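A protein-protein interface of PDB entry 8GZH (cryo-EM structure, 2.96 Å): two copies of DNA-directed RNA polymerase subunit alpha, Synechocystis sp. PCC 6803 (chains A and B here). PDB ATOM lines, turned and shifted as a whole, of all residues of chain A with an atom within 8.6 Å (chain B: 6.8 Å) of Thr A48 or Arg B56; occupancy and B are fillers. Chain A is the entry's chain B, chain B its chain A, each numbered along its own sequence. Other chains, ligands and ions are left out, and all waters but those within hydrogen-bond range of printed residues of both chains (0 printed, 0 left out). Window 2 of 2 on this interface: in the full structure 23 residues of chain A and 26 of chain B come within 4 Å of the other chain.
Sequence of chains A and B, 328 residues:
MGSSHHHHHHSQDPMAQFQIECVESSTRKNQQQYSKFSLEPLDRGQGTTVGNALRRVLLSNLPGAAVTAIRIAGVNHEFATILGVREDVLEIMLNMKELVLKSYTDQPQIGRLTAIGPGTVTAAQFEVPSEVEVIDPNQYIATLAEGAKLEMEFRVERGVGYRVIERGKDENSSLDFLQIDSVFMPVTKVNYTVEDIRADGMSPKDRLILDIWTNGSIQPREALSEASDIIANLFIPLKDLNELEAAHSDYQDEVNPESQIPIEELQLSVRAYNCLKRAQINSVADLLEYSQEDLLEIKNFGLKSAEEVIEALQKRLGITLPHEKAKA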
ATOM      1  N   LEU A  42     -26.314  -9.398   3.499  1.00  0.00           N
ATOM      2  CA  LEU A  42     -25.110 -10.096   3.916  1.00  0.00           C
ATOM      3  C   LEU A  42     -23.888  -9.339   3.418  1.00  0.00           C
ATOM      4  O   LEU A  42     -23.971  -8.518   2.502  1.00  0.00           O
ATOM      5  CB  LEU A  42     -25.097 -11.534   3.388  1.00  0.00           C
ATOM      6  CG  LEU A  42     -26.207 -12.452   3.902  1.00  0.00           C
ATOM      7  CD1 LEU A  42     -26.339 -13.688   3.036  1.00  0.00           C
ATOM      8  CD2 LEU A  42     -25.940 -12.841   5.340  1.00  0.00           C
ATOM      9  N   ASP A  43     -22.744  -9.618   4.034  1.00  0.00           N
ATOM     10  CA  ASP A  43     -21.504  -8.992   3.609  1.00  0.00           C
ATOM     11  C   ASP A  43     -20.993  -9.655   2.332  1.00  0.00           C
ATOM     12  O   ASP A  43     -21.565 -10.626   1.828  1.00  0.00           O
ATOM     13  CB  ASP A  43     -20.468  -9.052   4.729  1.00  0.00           C
ATOM     14  CG  ASP A  43     -20.828  -8.158   5.908  1.00  0.00           C
ATOM     15  OD1 ASP A  43     -21.812  -7.396   5.804  1.00  0.00           O
ATOM     16  OD2 ASP A  43     -20.128  -8.219   6.941  1.00  0.00           O
ATOM     17  N   ARG A  44     -19.899  -9.115   1.800  1.00  0.00           N
ATOM     18  CA  ARG A  44     -19.342  -9.586   0.538  1.00  0.00           C
ATOM     19  C   ARG A  44     -18.754 -10.980   0.716  1.00  0.00           C
ATOM     20  O   ARG A  44     -17.847 -11.181   1.530  1.00  0.00           O
ATOM     21  CB  ARG A  44     -18.277  -8.608   0.043  1.00  0.00           C
ATOM     22  CG  ARG A  44     -18.042  -8.609  -1.464  1.00  0.00           C
ATOM     23  CD  ARG A  44     -16.905  -9.539  -1.871  1.00  0.00           C
ATOM     24  NE  ARG A  44     -15.676  -9.281  -1.125  1.00  0.00           N
ATOM     25  CZ  ARG A  44     -14.740  -8.417  -1.500  1.00  0.00           C
ATOM     26  NH1 ARG A  44     -14.884  -7.725  -2.620  1.00  0.00           N
ATOM     27  NH2 ARG A  44     -13.655  -8.251  -0.755  1.00  0.00           N
ATOM     28  N   GLY A  45     -19.291 -11.948  -0.027  1.00  0.00           N
ATOM     29  CA  GLY A  45     -18.805 -13.305   0.009  1.00  0.00           C
ATOM     30  C   GLY A  45     -19.512 -14.227   0.977  1.00  0.00           C
ATOM     31  O   GLY A  45     -19.339 -15.446   0.876  1.00  0.00           O
ATOM     32  N   GLN A  46     -20.300 -13.692   1.910  1.00  0.00           N
ATOM     33  CA  GLN A  46     -20.969 -14.534   2.894  1.00  0.00           C
ATOM     34  C   GLN A  46     -22.183 -15.251   2.328  1.00  0.00           C
ATOM     35  O   GLN A  46     -22.577 -16.290   2.872  1.00  0.00           O
ATOM     36  CB  GLN A  46     -21.387 -13.704   4.107  1.00  0.00           C
ATOM     37  CG  GLN A  46     -20.324 -13.605   5.182  1.00  0.00           C
ATOM     38  CD  GLN A  46     -20.725 -12.685   6.311  1.00  0.00           C
ATOM     39  OE1 GLN A  46     -21.585 -11.825   6.149  1.00  0.00           O
ATOM     40  NE2 GLN A  46     -20.101 -12.860   7.467  1.00  0.00           N
ATOM     41  N   GLY A  47     -22.773 -14.727   1.252  1.00  0.00           N
ATOM     42  CA  GLY A  47     -23.927 -15.378   0.657  1.00  0.00           C
ATOM     43  C   GLY A  47     -23.590 -16.720   0.039  1.00  0.00           C
ATOM     44  O   GLY A  47     -24.346 -17.682   0.184  1.00  0.00           O
ATOM     45  N   THR A  48     -22.434 -16.807  -0.630  1.00  0.00           N
ATOM     46  CA  THR A  48     -21.973 -18.078  -1.180  1.00  0.00           C
ATOM     47  C   THR A  48     -21.673 -19.082  -0.075  1.00  0.00           C
ATOM     48  O   THR A  48     -21.984 -20.272  -0.212  1.00  0.00           O
ATOM     49  CB  THR A  48     -20.731 -17.855  -2.045  1.00  0.00           C
ATOM     50  OG1 THR A  48     -20.918 -16.693  -2.860  1.00  0.00           O
ATOM     51  CG2 THR A  48     -20.476 -19.054  -2.938  1.00  0.00           C
ATOM     52  N   THR A  49     -21.108 -18.609   1.039  1.00  0.00           N
ATOM     53  CA  THR A  49     -20.801 -19.472   2.177  1.00  0.00           C
ATOM     54  C   THR A  49     -22.067 -20.065   2.781  1.00  0.00           C
ATOM     55  O   THR A  49     -22.177 -21.291   2.947  1.00  0.00           O
ATOM     56  CB  THR A  49     -20.040 -18.672   3.235  1.00  0.00           C
ATOM     57  OG1 THR A  49     -19.016 -17.895   2.606  1.00  0.00           O
ATOM     58  CG2 THR A  49     -19.412 -19.597   4.253  1.00  0.00           C
ATOM     59  N   VAL A  50     -23.043 -19.203   3.090  1.00  0.00           N
ATOM     60  CA  VAL A  50     -24.293 -19.646   3.699  1.00  0.00           C
ATOM     61  C   VAL A  50     -25.079 -20.532   2.736  1.00  0.00           C
ATOM     62  O   VAL A  50     -25.613 -21.572   3.137  1.00  0.00           O
ATOM     63  CB  VAL A  50     -25.111 -18.426   4.165  1.00  0.00           C
ATOM     64  CG1 VAL A  50     -26.473 -18.838   4.684  1.00  0.00           C
ATOM     65  CG2 VAL A  50     -24.363 -17.675   5.245  1.00  0.00           C
ATOM     66  N   GLY A  51     -25.092 -20.184   1.446  1.00  0.00           N
ATOM     67  CA  GLY A  51     -25.840 -20.972   0.480  1.00  0.00           C
ATOM     68  C   GLY A  51     -25.247 -22.344   0.226  1.00  0.00           C
ATOM     69  O   GLY A  51     -25.979 -23.335   0.160  1.00  0.00           O
ATOM     70  N   ASN A  52     -23.917 -22.435   0.120  1.00  0.00           N
ATOM     71  CA  ASN A  52     -23.295 -23.731  -0.126  1.00  0.00           C
ATOM     72  C   ASN A  52     -23.363 -24.627   1.105  1.00  0.00           C
ATOM     73  O   ASN A  52     -23.618 -25.833   0.979  1.00  0.00           O
ATOM     74  CB  ASN A  52     -21.849 -23.546  -0.579  1.00  0.00           C
ATOM     75  CG  ASN A  52     -21.208 -24.847  -1.010  1.00  0.00           C
ATOM     76  OD1 ASN A  52     -21.597 -25.441  -2.014  1.00  0.00           O
ATOM     77  ND2 ASN A  52     -20.217 -25.297  -0.251  1.00  0.00           N
ATOM     78  N   ALA A  53     -23.171 -24.055   2.303  1.00  0.00           N
ATOM     79  CA  ALA A  53     -23.287 -24.851   3.521  1.00  0.00           C
ATOM     80  C   ALA A  53     -24.717 -25.331   3.741  1.00  0.00           C
ATOM     81  O   ALA A  53     -24.936 -26.499   4.095  1.00  0.00           O
ATOM     82  CB  ALA A  53     -22.798 -24.045   4.722  1.00  0.00           C
ATOM     83  N   LEU A  54     -25.702 -24.459   3.490  1.00  0.00           N
ATOM     84  CA  LEU A  54     -27.099 -24.843   3.639  1.00  0.00           C
ATOM     85  C   LEU A  54     -27.500 -25.890   2.614  1.00  0.00           C
ATOM     86  O   LEU A  54     -28.234 -26.823   2.947  1.00  0.00           O
ATOM     87  CB  LEU A  54     -28.000 -23.617   3.518  1.00  0.00           C
ATOM     88  CG  LEU A  54     -28.254 -22.817   4.791  1.00  0.00           C
ATOM     89  CD1 LEU A  54     -29.041 -21.564   4.462  1.00  0.00           C
ATOM     90  CD2 LEU A  54     -28.979 -23.658   5.818  1.00  0.00           C
ATOM     91  N   ARG A  55     -27.001 -25.777   1.378  1.00  0.00           N
ATOM     92  CA  ARG A  55     -27.321 -26.764   0.354  1.00  0.00           C
ATOM     93  C   ARG A  55     -26.732 -28.129   0.688  1.00  0.00           C
ATOM     94  O   ARG A  55     -27.422 -29.151   0.563  1.00  0.00           O
ATOM     95  CB  ARG A  55     -26.822 -26.288  -1.008  1.00  0.00           C
ATOM     96  CG  ARG A  55     -27.236 -27.194  -2.145  1.00  0.00           C
ATOM     97  CD  ARG A  55     -26.571 -26.818  -3.447  1.00  0.00           C
ATOM     98  NE  ARG A  55     -27.105 -27.607  -4.552  1.00  0.00           N
ATOM     99  CZ  ARG A  55     -26.655 -28.807  -4.900  1.00  0.00           C
ATOM    100  NH1 ARG A  55     -25.649 -29.359  -4.238  1.00  0.00           N
ATOM    101  NH2 ARG A  55     -27.207 -29.453  -5.916  1.00  0.00           N
ATOM    102  N   TYR A 192     -29.511 -22.029  -5.217  1.00  0.00           N
ATOM    103  CA  TYR A 192     -29.269 -20.723  -4.622  1.00  0.00           C
ATOM    104  C   TYR A 192     -28.537 -19.824  -5.607  1.00  0.00           C
ATOM    105  O   TYR A 192     -27.639 -20.275  -6.323  1.00  0.00           O
ATOM    106  CB  TYR A 192     -28.486 -20.840  -3.302  1.00  0.00           C
ATOM    107  CG  TYR A 192     -27.028 -21.219  -3.433  1.00  0.00           C
ATOM    108  CD1 TYR A 192     -26.649 -22.541  -3.610  1.00  0.00           C
ATOM    109  CD2 TYR A 192     -26.031 -20.253  -3.361  1.00  0.00           C
ATOM    110  CE1 TYR A 192     -25.319 -22.889  -3.727  1.00  0.00           C
ATOM    111  CE2 TYR A 192     -24.704 -20.591  -3.478  1.00  0.00           C
ATOM    112  CZ  TYR A 192     -24.353 -21.909  -3.659  1.00  0.00           C
ATOM    113  OH  TYR A 192     -23.026 -22.246  -3.772  1.00  0.00           O
ATOM    114  N   THR A 193     -28.952 -18.556  -5.661  1.00  0.00           N
ATOM    115  CA  THR A 193     -28.259 -17.514  -6.407  1.00  0.00           C
ATOM    116  C   THR A 193     -27.992 -16.337  -5.479  1.00  0.00           C
ATOM    117  O   THR A 193     -28.761 -16.074  -4.553  1.00  0.00           O
ATOM    118  CB  THR A 193     -29.054 -17.008  -7.637  1.00  0.00           C
ATOM    119  OG1 THR A 193     -30.078 -16.099  -7.212  1.00  0.00           O
ATOM    120  CG2 THR A 193     -29.680 -18.151  -8.430  1.00  0.00           C
ATOM    121  N   VAL A 194     -26.898 -15.627  -5.737  1.00  0.00           N
ATOM    122  CA  VAL A 194     -26.495 -14.468  -4.946  1.00  0.00           C
ATOM    123  C   VAL A 194     -26.627 -13.224  -5.813  1.00  0.00           C
ATOM    124  O   VAL A 194     -26.195 -13.219  -6.971  1.00  0.00           O
ATOM    125  CB  VAL A 194     -25.060 -14.616  -4.411  1.00  0.00           C
ATOM    126  CG1 VAL A 194     -24.791 -13.599  -3.322  1.00  0.00           C
ATOM    127  CG2 VAL A 194     -24.826 -16.021  -3.892  1.00  0.00           C
ATOM    128  N   GLU A 195     -27.222 -12.172  -5.252  1.00  0.00           N
ATOM    129  CA  GLU A 195     -27.410 -10.904  -5.943  1.00  0.00           C
ATOM    130  C   GLU A 195     -26.638  -9.807  -5.223  1.00  0.00           C
ATOM    131  O   GLU A 195     -26.603  -9.769  -3.989  1.00  0.00           O
ATOM    132  CB  GLU A 195     -28.894 -10.527  -6.022  1.00  0.00           C
ATOM    133  CG  GLU A 195     -29.710 -11.397  -6.960  1.00  0.00           C
ATOM    134  CD  GLU A 195     -31.146 -10.926  -7.093  1.00  0.00           C
ATOM    135  OE1 GLU A 195     -31.595 -10.128  -6.242  1.00  0.00           O
ATOM    136  OE2 GLU A 195     -31.828 -11.353  -8.048  1.00  0.00           O
ATOM    137  N   ASP A 206     -24.535  -8.357  -0.170  1.00  0.00           N
ATOM    138  CA  ASP A 206     -24.973  -9.568  -0.845  1.00  0.00           C
ATOM    139  C   ASP A 206     -26.400  -9.898  -0.438  1.00  0.00           C
ATOM    140  O   ASP A 206     -26.791  -9.692   0.713  1.00  0.00           O
ATOM    141  CB  ASP A 206     -24.056 -10.752  -0.514  1.00  0.00           C
ATOM    142  CG  ASP A 206     -22.880 -10.866  -1.465  1.00  0.00           C
ATOM    143  OD1 ASP A 206     -23.010 -10.447  -2.633  1.00  0.00           O
ATOM    144  OD2 ASP A 206     -21.825 -11.382  -1.044  1.00  0.00           O
ATOM    145  N   ARG A 207     -27.170 -10.419  -1.390  1.00  0.00           N
ATOM    146  CA  ARG A 207     -28.523 -10.900  -1.146  1.00  0.00           C
ATOM    147  C   ARG A 207     -28.600 -12.358  -1.574  1.00  0.00           C
ATOM    148  O   ARG A 207     -28.316 -12.684  -2.729  1.00  0.00           O
ATOM    149  CB  ARG A 207     -29.551 -10.060  -1.902  1.00  0.00           C
ATOM    150  CG  ARG A 207     -30.944 -10.651  -1.909  1.00  0.00           C
ATOM    151  CD  ARG A 207     -31.867  -9.864  -2.818  1.00  0.00           C
ATOM    152  NE  ARG A 207     -32.019  -8.485  -2.368  1.00  0.00           N
ATOM    153  CZ  ARG A 207     -31.662  -7.421  -3.079  1.00  0.00           C
ATOM    154  NH1 ARG A 207     -31.134  -7.570  -4.285  1.00  0.00           N
ATOM    155  NH2 ARG A 207     -31.835  -6.206  -2.582  1.00  0.00           N
ATOM    156  N   LEU A 208     -28.981 -13.230  -0.647  1.00  0.00           N
ATOM    157  CA  LEU A 208     -29.048 -14.662  -0.901  1.00  0.00           C
ATOM    158  C   LEU A 208     -30.479 -15.051  -1.252  1.00  0.00           C
ATOM    159  O   LEU A 208     -31.399 -14.825  -0.461  1.00  0.00           O
ATOM    160  CB  LEU A 208     -28.559 -15.454   0.309  1.00  0.00           C
ATOM    161  CG  LEU A 208     -28.522 -16.976   0.154  1.00  0.00           C
ATOM    162  CD1 LEU A 208     -27.527 -17.384  -0.914  1.00  0.00           C
ATOM    163  CD2 LEU A 208     -28.192 -17.640   1.479  1.00  0.00           C
ATOM    164  N   ILE A 209     -30.659 -15.628  -2.435  1.00  0.00           N
ATOM    165  CA  ILE A 209     -31.950 -16.124  -2.900  1.00  0.00           C
ATOM    166  C   ILE A 209     -31.897 -17.643  -2.864  1.00  0.00           C
ATOM    167  O   ILE A 209     -31.114 -18.256  -3.593  1.00  0.00           O
ATOM    168  CB  ILE A 209     -32.276 -15.620  -4.313  1.00  0.00           C
ATOM    169  CG1 ILE A 209     -32.378 -14.097  -4.329  1.00  0.00           C
ATOM    170  CG2 ILE A 209     -33.566 -16.242  -4.812  1.00  0.00           C
ATOM    171  CD1 ILE A 209     -33.458 -13.556  -3.429  1.00  0.00           C
ATOM    172  N   GLY B  51     -14.756 -27.088   6.724  1.00  0.00           N
ATOM    173  CA  GLY B  51     -13.481 -26.590   6.240  1.00  0.00           C
ATOM    174  C   GLY B  51     -13.617 -25.441   5.262  1.00  0.00           C
ATOM    175  O   GLY B  51     -12.897 -24.446   5.366  1.00  0.00           O
ATOM    176  N   ASN B  52     -14.566 -25.537   4.324  1.00  0.00           N
ATOM    177  CA  ASN B  52     -14.708 -24.476   3.335  1.00  0.00           C
ATOM    178  C   ASN B  52     -15.336 -23.226   3.939  1.00  0.00           C
ATOM    179  O   ASN B  52     -14.948 -22.106   3.579  1.00  0.00           O
ATOM    180  CB  ASN B  52     -15.526 -24.961   2.144  1.00  0.00           C
ATOM    181  CG  ASN B  52     -15.420 -24.030   0.958  1.00  0.00           C
ATOM    182  OD1 ASN B  52     -16.424 -23.516   0.467  1.00  0.00           O
ATOM    183  ND2 ASN B  52     -14.201 -23.797   0.499  1.00  0.00           N
ATOM    184  N   ALA B  53     -16.279 -23.388   4.878  1.00  0.00           N
ATOM    185  CA  ALA B  53     -16.846 -22.222   5.551  1.00  0.00           C
ATOM    186  C   ALA B  53     -15.805 -21.520   6.413  1.00  0.00           C
ATOM    187  O   ALA B  53     -15.716 -20.283   6.404  1.00  0.00           O
ATOM    188  CB  ALA B  53     -18.051 -22.637   6.393  1.00  0.00           C
ATOM    189  N   LEU B  54     -14.978 -22.297   7.124  1.00  0.00           N
ATOM    190  CA  LEU B  54     -13.907 -21.718   7.928  1.00  0.00           C
ATOM    191  C   LEU B  54     -12.866 -21.028   7.060  1.00  0.00           C
ATOM    192  O   LEU B  54     -12.392 -19.947   7.413  1.00  0.00           O
ATOM    193  CB  LEU B  54     -13.252 -22.798   8.784  1.00  0.00           C
ATOM    194  CG  LEU B  54     -13.900 -23.068  10.138  1.00  0.00           C
ATOM    195  CD1 LEU B  54     -13.221 -24.241  10.811  1.00  0.00           C
ATOM    196  CD2 LEU B  54     -13.832 -21.836  11.009  1.00  0.00           C
ATOM    197  N   ARG B  55     -12.526 -21.618   5.908  1.00  0.00           N
ATOM    198  CA  ARG B  55     -11.531 -21.012   5.027  1.00  0.00           C
ATOM    199  C   ARG B  55     -12.033 -19.705   4.427  1.00  0.00           C
ATOM    200  O   ARG B  55     -11.299 -18.708   4.408  1.00  0.00           O
ATOM    201  CB  ARG B  55     -11.141 -21.986   3.918  1.00  0.00           C
ATOM    202  CG  ARG B  55     -10.126 -21.411   2.958  1.00  0.00           C
ATOM    203  CD  ARG B  55      -9.694 -22.400   1.906  1.00  0.00           C
ATOM    204  NE  ARG B  55      -8.565 -21.888   1.137  1.00  0.00           N
ATOM    205  CZ  ARG B  55      -8.679 -21.095   0.079  1.00  0.00           C
ATOM    206  NH1 ARG B  55      -9.874 -20.720  -0.350  1.00  0.00           N
ATOM    207  NH2 ARG B  55      -7.594 -20.677  -0.553  1.00  0.00           N
ATOM    208  N   ARG B  56     -13.290 -19.681   3.964  1.00  0.00           N
ATOM    209  CA  ARG B  56     -13.836 -18.466   3.367  1.00  0.00           C
ATOM    210  C   ARG B  56     -13.980 -17.349   4.396  1.00  0.00           C
ATOM    211  O   ARG B  56     -13.627 -16.197   4.112  1.00  0.00           O
ATOM    212  CB  ARG B  56     -15.179 -18.764   2.703  1.00  0.00           C
ATOM    213  CG  ARG B  56     -15.066 -19.593   1.441  1.00  0.00           C
ATOM    214  CD  ARG B  56     -16.413 -19.795   0.780  1.00  0.00           C
ATOM    215  NE  ARG B  56     -17.048 -18.524   0.451  1.00  0.00           N
ATOM    216  CZ  ARG B  56     -16.828 -17.845  -0.667  1.00  0.00           C
ATOM    217  NH1 ARG B  56     -15.990 -18.313  -1.576  1.00  0.00           N
ATOM    218  NH2 ARG B  56     -17.447 -16.695  -0.877  1.00  0.00           N
ATOM    219  N   VAL B  57     -14.438 -17.674   5.611  1.00  0.00           N
ATOM    220  CA  VAL B  57     -14.594 -16.641   6.632  1.00  0.00           C
ATOM    221  C   VAL B  57     -13.234 -16.164   7.141  1.00  0.00           C
ATOM    222  O   VAL B  57     -13.020 -14.960   7.323  1.00  0.00           O
ATOM    223  CB  VAL B  57     -15.504 -17.156   7.764  1.00  0.00           C
ATOM    224  CG1 VAL B  57     -15.515 -16.207   8.950  1.00  0.00           C
ATOM    225  CG2 VAL B  57     -16.912 -17.325   7.241  1.00  0.00           C
ATOM    226  N   LEU B  58     -12.274 -17.081   7.313  1.00  0.00           N
ATOM    227  CA  LEU B  58     -10.943 -16.704   7.779  1.00  0.00           C
ATOM    228  C   LEU B  58     -10.180 -15.888   6.746  1.00  0.00           C
ATOM    229  O   LEU B  58      -9.328 -15.075   7.114  1.00  0.00           O
ATOM    230  CB  LEU B  58     -10.143 -17.954   8.139  1.00  0.00           C
ATOM    231  CG  LEU B  58     -10.272 -18.495   9.558  1.00  0.00           C
ATOM    232  CD1 LEU B  58      -9.828 -19.940   9.606  1.00  0.00           C
ATOM    233  CD2 LEU B  58      -9.467 -17.656  10.522  1.00  0.00           C
ATOM    234  N   LEU B  59     -10.459 -16.084   5.461  1.00  0.00           N
ATOM    235  CA  LEU B  59      -9.785 -15.304   4.437  1.00  0.00           C
ATOM    236  C   LEU B  59     -10.495 -14.001   4.100  1.00  0.00           C
ATOM    237  O   LEU B  59      -9.845 -13.082   3.594  1.00  0.00           O
ATOM    238  CB  LEU B  59      -9.623 -16.131   3.160  1.00  0.00           C
ATOM    239  CG  LEU B  59      -8.528 -17.196   3.152  1.00  0.00           C
ATOM    240  CD1 LEU B  59      -8.388 -17.789   1.766  1.00  0.00           C
ATOM    241  CD2 LEU B  59      -7.207 -16.623   3.630  1.00  0.00           C
ATOM    242  N   SER B  60     -11.797 -13.882   4.367  1.00  0.00           N
ATOM    243  CA  SER B  60     -12.533 -12.700   3.942  1.00  0.00           C
ATOM    244  C   SER B  60     -12.985 -11.793   5.079  1.00  0.00           C
ATOM    245  O   SER B  60     -12.886 -10.570   4.955  1.00  0.00           O
ATOM    246  CB  SER B  60     -13.751 -13.123   3.110  1.00  0.00           C
ATOM    247  OG  SER B  60     -14.540 -14.075   3.797  1.00  0.00           O
ATOM    248  N   ASN B  61     -13.484 -12.342   6.184  1.00  0.00           N
ATOM    249  CA  ASN B  61     -14.247 -11.564   7.156  1.00  0.00           C
ATOM    250  C   ASN B  61     -13.572 -11.469   8.522  1.00  0.00           C
ATOM    251  O   ASN B  61     -14.223 -11.630   9.555  1.00  0.00           O
ATOM    252  CB  ASN B  61     -15.649 -12.144   7.321  1.00  0.00           C
ATOM    253  CG  ASN B  61     -16.341 -12.383   6.002  1.00  0.00           C
ATOM    254  OD1 ASN B  61     -16.911 -13.448   5.776  1.00  0.00           O
ATOM    255  ND2 ASN B  61     -16.306 -11.391   5.125  1.00  0.00           N
ATOM    256  N   VAL B 190      -5.045 -20.185   4.389  1.00  0.00           N
ATOM    257  CA  VAL B 190      -5.761 -21.278   5.038  1.00  0.00           C
ATOM    258  C   VAL B 190      -5.715 -22.485   4.112  1.00  0.00           C
ATOM    259  O   VAL B 190      -5.974 -22.358   2.911  1.00  0.00           O
ATOM    260  CB  VAL B 190      -7.222 -20.906   5.364  1.00  0.00           C
ATOM    261  CG1 VAL B 190      -7.880 -21.993   6.190  1.00  0.00           C
ATOM    262  CG2 VAL B 190      -7.303 -19.585   6.096  1.00  0.00           C
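The guanidinium group (NE) of Arg B56 is in hydrogen-bond range of the side-chain hydroxyl (OG1) of Thr A49 (3.0 Å). The guanidinium group (NH2) of Arg B56 is in hydrogen-bond range of the backbone carbonyl oxygen (O) of Gly A45 (2.9 Å).
The backbone NH (N) of Gly A45 sits at hydrogen-bond distance from the side-chain carboxylate (OD2) of Asp A206. The backbone carbonyl oxygen of Gly A45 is in hydrogen-bond range of the side-chain hydroxyl of Thr A49, at 3.0 Å. The side-chain amide oxygen (OD1) of Asn B61 is in hydrogen-bond range of the side-chain hydroxyl (OG) of Ser B60, 3.2 Å away. The backbone NH of Asp A43 lies within hydrogen-bond range of the side-chain amide oxygen of Gln A46 (3.3 Å).
Among the printed residues, pairs that only touch across the chains: Arg A44 with Asn B61 (3.9 Å), Gln A46 with Asn B61 (3.5 Å), Thr A48 with Arg B56 (3.7 Å) and Thr A49 with Ala B53 (3.9 Å).
Of the printed residues of chain B, Arg A44 touches Asn B61 (3.9 Å). Of the printed residues of chain B, Gln A46 touches Asn B61 (3.5 Å). Thr A48 touches just one residue of chain B: Arg B56 (3.7 Å). Printed residues of chain A within 4 Å of Ala B53: Thr A49. Arg B56 touches just these residues of chain A: Gly A45 (2.9 Å), Thr A48 (3.7 Å) and Thr A49 (3.0 Å). Printed residues of chain A within 4 Å of Asn B61: Arg A44 (3.9 Å) and Gln A46 (3.5 Å).
Hydrophobic or aromatic side chains of chain B within 4 Å of the printed part of chain A: Ala B53.
Positions printed for both chains: 51, 52, 53, 54 and 55. Of the 6 pairs that touch across the chains among the printed residues, none has its exchanged pair printed and touching as well.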
